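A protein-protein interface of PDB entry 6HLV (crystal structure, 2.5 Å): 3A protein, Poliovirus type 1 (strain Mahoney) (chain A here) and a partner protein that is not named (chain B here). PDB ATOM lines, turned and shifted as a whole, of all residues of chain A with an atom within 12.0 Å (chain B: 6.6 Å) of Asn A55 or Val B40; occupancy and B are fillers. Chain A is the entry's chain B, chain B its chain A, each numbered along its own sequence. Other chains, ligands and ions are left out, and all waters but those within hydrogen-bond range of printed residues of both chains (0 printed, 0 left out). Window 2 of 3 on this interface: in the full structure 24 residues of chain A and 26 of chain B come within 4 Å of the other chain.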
ATOM      1  N   GLN A  51     -17.153  12.926  -0.616  1.00  0.00           N
ATOM      2  CA  GLN A  51     -17.390  11.989  -1.717  1.00  0.00           C
ATOM      3  C   GLN A  51     -17.260  12.727  -3.042  1.00  0.00           C
ATOM      4  O   GLN A  51     -17.588  13.909  -3.122  1.00  0.00           O
ATOM      5  CB  GLN A  51     -18.779  11.357  -1.629  1.00  0.00           C
ATOM      6  CG  GLN A  51     -18.946  10.269  -0.593  1.00  0.00           C
ATOM      7  CD  GLN A  51     -20.338   9.664  -0.631  1.00  0.00           C
ATOM      8  OE1 GLN A  51     -21.100   9.895  -1.570  1.00  0.00           O
ATOM      9  NE2 GLN A  51     -20.676   8.884   0.388  1.00  0.00           N
ATOM     10  N   THR A  52     -16.781  12.039  -4.076  1.00  0.00           N
ATOM     11  CA  THR A  52     -16.717  12.625  -5.415  1.00  0.00           C
ATOM     12  C   THR A  52     -17.534  11.826  -6.427  1.00  0.00           C
ATOM     13  O   THR A  52     -17.518  10.594  -6.433  1.00  0.00           O
ATOM     14  CB  THR A  52     -15.272  12.731  -5.924  1.00  0.00           C
ATOM     15  OG1 THR A  52     -14.727  11.422  -6.123  1.00  0.00           O
ATOM     16  CG2 THR A  52     -14.415  13.504  -4.935  1.00  0.00           C
ATOM     17  N   GLU A  53     -18.242  12.559  -7.280  1.00  0.00           N
ATOM     18  CA  GLU A  53     -19.076  11.993  -8.332  1.00  0.00           C
ATOM     19  C   GLU A  53     -18.714  12.662  -9.657  1.00  0.00           C
ATOM     20  O   GLU A  53     -18.703  13.889  -9.747  1.00  0.00           O
ATOM     21  CB  GLU A  53     -20.558  12.189  -7.988  1.00  0.00           C
ATOM     22  CG  GLU A  53     -21.539  12.042  -9.144  1.00  0.00           C
ATOM     23  CD  GLU A  53     -22.930  12.524  -8.779  1.00  0.00           C
ATOM     24  OE1 GLU A  53     -23.223  12.640  -7.569  1.00  0.00           O
ATOM     25  OE2 GLU A  53     -23.727  12.799  -9.700  1.00  0.00           O
ATOM     26  N   ARG A  54     -18.420  11.855 -10.673  1.00  0.00           N
ATOM     27  CA  ARG A  54     -17.941  12.363 -11.959  1.00  0.00           C
ATOM     28  C   ARG A  54     -18.874  11.993 -13.109  1.00  0.00           C
ATOM     29  O   ARG A  54     -19.031  10.817 -13.438  1.00  0.00           O
ATOM     30  CB  ARG A  54     -16.535  11.827 -12.239  1.00  0.00           C
ATOM     31  CG  ARG A  54     -15.879  12.401 -13.483  1.00  0.00           C
ATOM     32  CD  ARG A  54     -14.561  11.704 -13.783  1.00  0.00           C
ATOM     33  NE  ARG A  54     -13.631  11.764 -12.655  1.00  0.00           N
ATOM     34  CZ  ARG A  54     -12.671  12.674 -12.506  1.00  0.00           C
ATOM     35  NH1 ARG A  54     -12.487  13.626 -13.413  1.00  0.00           N
ATOM     36  NH2 ARG A  54     -11.885  12.630 -11.440  1.00  0.00           N
ATOM     37  N   ASN A  55     -19.478  13.005 -13.725  1.00  0.00           N
ATOM     38  CA  ASN A  55     -20.413  12.802 -14.828  1.00  0.00           C
ATOM     39  C   ASN A  55     -19.923  13.428 -16.129  1.00  0.00           C
ATOM     40  O   ASN A  55     -19.103  14.345 -16.118  1.00  0.00           O
ATOM     41  CB  ASN A  55     -21.787  13.374 -14.472  1.00  0.00           C
ATOM     42  CG  ASN A  55     -22.513  12.546 -13.431  1.00  0.00           C
ATOM     43  OD1 ASN A  55     -22.932  13.061 -12.395  1.00  0.00           O
ATOM     44  ND2 ASN A  55     -22.669  11.255 -13.703  1.00  0.00           N
ATOM     45  N   ILE A  56     -20.430  12.916 -17.248  1.00  0.00           N
ATOM     46  CA  ILE A  56     -20.106  13.449 -18.567  1.00  0.00           C
ATOM     47  C   ILE A  56     -21.377  13.650 -19.385  1.00  0.00           C
ATOM     48  O   ILE A  56     -21.657  14.753 -19.851  1.00  0.00           O
ATOM     49  CB  ILE A  56     -19.153  12.522 -19.343  1.00  0.00           C
ATOM     50  CG1 ILE A  56     -17.998  12.064 -18.447  1.00  0.00           C
ATOM     51  CG2 ILE A  56     -18.622  13.226 -20.581  1.00  0.00           C
ATOM     52  CD1 ILE A  56     -18.252  10.750 -17.731  1.00  0.00           C
ATOM     53  N   VAL B  35     -10.312  17.686 -13.691  1.00  0.00           N
ATOM     54  CA  VAL B  35     -11.619  17.634 -14.335  1.00  0.00           C
ATOM     55  C   VAL B  35     -11.425  17.505 -15.839  1.00  0.00           C
ATOM     56  O   VAL B  35     -10.844  18.384 -16.475  1.00  0.00           O
ATOM     57  CB  VAL B  35     -12.467  18.883 -14.028  1.00  0.00           C
ATOM     58  CG1 VAL B  35     -13.885  18.706 -14.549  1.00  0.00           C
ATOM     59  CG2 VAL B  35     -12.483  19.161 -12.537  1.00  0.00           C
ATOM     60  N   GLY B  36     -11.909  16.404 -16.404  1.00  0.00           N
ATOM     61  CA  GLY B  36     -11.710  16.121 -17.813  1.00  0.00           C
ATOM     62  C   GLY B  36     -12.464  17.057 -18.736  1.00  0.00           C
ATOM     63  O   GLY B  36     -13.277  17.873 -18.298  1.00  0.00           O
ATOM     64  N   GLY B  38     -15.254  18.298 -20.872  1.00  0.00           N
ATOM     65  CA  GLY B  38     -16.682  18.039 -20.903  1.00  0.00           C
ATOM     66  C   GLY B  38     -17.216  17.370 -19.649  1.00  0.00           C
ATOM     67  O   GLY B  38     -18.353  16.899 -19.633  1.00  0.00           O
ATOM     68  N   GLU B  39     -16.406  17.345 -18.594  1.00  0.00           N
ATOM     69  CA  GLU B  39     -16.755  16.641 -17.361  1.00  0.00           C
ATOM     70  C   GLU B  39     -17.251  17.574 -16.265  1.00  0.00           C
ATOM     71  O   GLU B  39     -16.837  18.730 -16.178  1.00  0.00           O
ATOM     72  CB  GLU B  39     -15.551  15.857 -16.836  1.00  0.00           C
ATOM     73  CG  GLU B  39     -15.327  14.523 -17.523  1.00  0.00           C
ATOM     74  CD  GLU B  39     -14.166  13.749 -16.932  1.00  0.00           C
ATOM     75  OE1 GLU B  39     -13.507  14.272 -16.007  1.00  0.00           O
ATOM     76  OE2 GLU B  39     -13.913  12.616 -17.392  1.00  0.00           O
ATOM     77  N   VAL B  40     -18.163  17.059 -15.446  1.00  0.00           N
ATOM     78  CA  VAL B  40     -18.582  17.727 -14.221  1.00  0.00           C
ATOM     79  C   VAL B  40     -18.258  16.847 -13.020  1.00  0.00           C
ATOM     80  O   VAL B  40     -18.765  15.733 -12.908  1.00  0.00           O
ATOM     81  CB  VAL B  40     -20.086  18.043 -14.224  1.00  0.00           C
ATOM     82  CG1 VAL B  40     -20.510  18.620 -12.883  1.00  0.00           C
ATOM     83  CG2 VAL B  40     -20.426  19.000 -15.355  1.00  0.00           C
ATOM     84  N   VAL B  41     -17.406  17.351 -12.133  1.00  0.00           N
ATOM     85  CA  VAL B  41     -17.082  16.659 -10.890  1.00  0.00           C
ATOM     86  C   VAL B  41     -17.829  17.308  -9.732  1.00  0.00           C
ATOM     87  O   VAL B  41     -17.708  18.512  -9.503  1.00  0.00           O
ATOM     88  CB  VAL B  41     -15.567  16.676 -10.598  1.00  0.00           C
ATOM     89  CG1 VAL B  41     -15.283  16.091  -9.225  1.00  0.00           C
ATOM     90  CG2 VAL B  41     -14.807  15.909 -11.673  1.00  0.00           C
ATOM     91  N   THR B  42     -18.602  16.503  -9.012  1.00  0.00           N
ATOM     92  CA  THR B  42     -19.385  16.987  -7.882  1.00  0.00           C
ATOM     93  C   THR B  42     -18.761  16.528  -6.570  1.00  0.00           C
ATOM     94  O   THR B  42     -18.621  15.331  -6.326  1.00  0.00           O
ATOM     95  CB  THR B  42     -20.845  16.497  -7.952  1.00  0.00           C
ATOM     96  OG1 THR B  42     -21.424  16.876  -9.207  1.00  0.00           O
ATOM     97  CG2 THR B  42     -21.665  17.095  -6.824  1.00  0.00           C
ATOM     98  N   LYS B 145     -20.010  22.019  -7.237  1.00  0.00           N
ATOM     99  CA  LYS B 145     -19.928  21.655  -8.644  1.00  0.00           C
ATOM    100  C   LYS B 145     -18.716  22.287  -9.293  1.00  0.00           C
ATOM    101  O   LYS B 145     -18.613  23.506  -9.344  1.00  0.00           O
ATOM    102  CB  LYS B 145     -21.189  22.097  -9.387  1.00  0.00           C
ATOM    103  CG  LYS B 145     -22.454  21.375  -8.971  1.00  0.00           C
ATOM    104  CD  LYS B 145     -22.489  19.964  -9.520  1.00  0.00           C
ATOM    105  CE  LYS B 145     -23.835  19.311  -9.276  1.00  0.00           C
ATOM    106  NZ  LYS B 145     -23.842  17.885  -9.698  1.00  0.00           N
ATOM    107  N   PHE B 146     -17.796  21.463  -9.781  1.00  0.00           N
ATOM    108  CA  PHE B 146     -16.735  21.958 -10.645  1.00  0.00           C
ATOM    109  C   PHE B 146     -17.071  21.530 -12.064  1.00  0.00           C
ATOM    110  O   PHE B 146     -16.943  20.361 -12.427  1.00  0.00           O
ATOM    111  CB  PHE B 146     -15.373  21.439 -10.184  1.00  0.00           C
ATOM    112  CG  PHE B 146     -14.990  21.931  -8.818  1.00  0.00           C
ATOM    113  CD1 PHE B 146     -14.571  23.237  -8.635  1.00  0.00           C
ATOM    114  CD2 PHE B 146     -15.078  21.101  -7.715  1.00  0.00           C
ATOM    115  CE1 PHE B 146     -14.234  23.701  -7.381  1.00  0.00           C
ATOM    116  CE2 PHE B 146     -14.742  21.561  -6.459  1.00  0.00           C
ATOM    117  CZ  PHE B 146     -14.319  22.863  -6.293  1.00  0.00           C
ATOM    118  N   ASP B 147     -17.494  22.506 -12.860  1.00  0.00           N
ATOM    119  CA  ASP B 147     -18.166  22.231 -14.122  1.00  0.00           C
ATOM    120  C   ASP B 147     -17.294  22.634 -15.301  1.00  0.00           C
ATOM    121  O   ASP B 147     -17.129  23.817 -15.599  1.00  0.00           O
ATOM    122  CB  ASP B 147     -19.504  22.978 -14.151  1.00  0.00           C
ATOM    123  CG  ASP B 147     -20.440  22.475 -15.232  1.00  0.00           C
ATOM    124  OD1 ASP B 147     -19.967  22.143 -16.335  1.00  0.00           O
ATOM    125  OD2 ASP B 147     -21.658  22.416 -14.971  1.00  0.00           O
ATOM    126  N   ASN B 148     -16.731  21.625 -15.957  1.00  0.00           N
ATOM    127  CA  ASN B 148     -15.908  21.805 -17.145  1.00  0.00           C
ATOM    128  C   ASN B 148     -16.658  21.502 -18.443  1.00  0.00           C
ATOM    129  O   ASN B 148     -16.059  21.480 -19.514  1.00  0.00           O
ATOM    130  CB  ASN B 148     -14.656  20.935 -17.049  1.00  0.00           C
ATOM    131  CG  ASN B 148     -13.540  21.424 -17.942  1.00  0.00           C
ATOM    132  OD1 ASN B 148     -13.364  22.626 -18.132  1.00  0.00           O
ATOM    133  ND2 ASN B 148     -12.784  20.494 -18.506  1.00  0.00           N
ATOM    134  N   SER B 149     -17.954  21.237 -18.338  1.00  0.00           N
ATOM    135  CA  SER B 149     -18.736  20.690 -19.449  1.00  0.00           C
ATOM    136  C   SER B 149     -18.669  21.511 -20.741  1.00  0.00           C
ATOM    137  O   SER B 149     -18.952  20.997 -21.822  1.00  0.00           O
ATOM    138  CB  SER B 149     -20.196  20.548 -19.027  1.00  0.00           C
ATOM    139  OG  SER B 149     -20.718  21.789 -18.594  1.00  0.00           O
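N of Gly B36 lies within hydrogen-bond range of OE1 of Glu B39, at 2.7 Å. The backbone carbonyl oxygen of Val B41 lies within hydrogen-bond range of the backbone NH of Phe B146 (3.0 Å). The backbone NH (N) of Asn B148 is in hydrogen-bond range of the backbone carbonyl oxygen (O) of Glu B39 (2.9 Å). The backbone NH of Ser B149 sits at hydrogen-bond distance from the backbone carbonyl oxygen of Glu B39 (3.5 Å). The side-chain carboxylate (OE2) of Glu A53 lies close to the side-chain amide oxygen (OD1) of Asn A55, 2.8 Å away. The side-chain amino group (NZ) of Lys B145 sits at hydrogen-bond distance from the side-chain hydroxyl (OG1) of Thr B42, 2.7 Å away.
Gln A51 touches Thr B42 (O to O, 3.7 Å). Thr B42 touches Thr A52. Val B40 touches Glu A53. Val B41 touches Glu A53 (CA to O, 3.4 Å). Arg A54 touches Val B40 (CA to O, 3.6 Å). CG2 of Val B41 touches NH1 of Arg A54, 3.7 Å away. Asn A55 touches Glu B39. O of Gly B38 touches CG2 of Ile A56 (3.8 Å). Glu B39 touches Ile A56.
OE1 of Glu B39 lies within salt-bridge range of NH1 of Arg A54, 2.9 Å away. N of Asn A55 lies within hydrogen-bond range of O of Val B40 (2.9 Å). O of Glu A53 lies within hydrogen-bond range of N of Thr B42, at 2.7 Å.
Printed residues of chain B within 4 Å of Gln A51: Thr B42. Of the printed residues of chain B, Arg A54 touches Glu B39 (2.9 Å), Val B40 (3.6 Å) and Val B41 (3.7 Å). Of chain B, only Glu B39 (3.5 Å) and Val B40 (2.9 Å) come within 4 Å of Asn A55. Of the printed residues of chain B, Ile A56 touches Gly B38 (3.8 Å) and Glu B39 (3.7 Å). Val B35 touches none of the printed residues of chain A. No residue of chain A comes within 4 Å of Gly B36. Gly B38 touches one residue of chain A. Val B41 touches just these residues of chain A: Glu A53 and Arg A54. Of the printed residues of chain A, Thr B42 touches Gln A51 (3.7 Å), Thr A52 (3.4 Å) and Glu A53 (2.7 Å). No residue of chain A comes within 4 Å of Lys B145. Phe B146 touches none of the printed residues of chain A. No residue of chain A comes within 4 Å of Asp B147. No residue of chain A comes within 4 Å of Asn B148. No residue of chain A comes within 4 Å of Ser B149. The nearest residue of chain B that does not touch Asn A55 is Gly B38 (4.4 Å).
Printed residues of chain A that touch a printed residue of chain B: Gln A51, Thr A52, Glu A53, Arg A54, Asn A55 and Ile A56. Among the printed residues, 12 pairs touch across the chains. Among the printed residues, Asp or Glu carboxylates within 4 Å of a Lys or Arg side-chain nitrogen of the other chain: Arg A54 with Glu B39.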
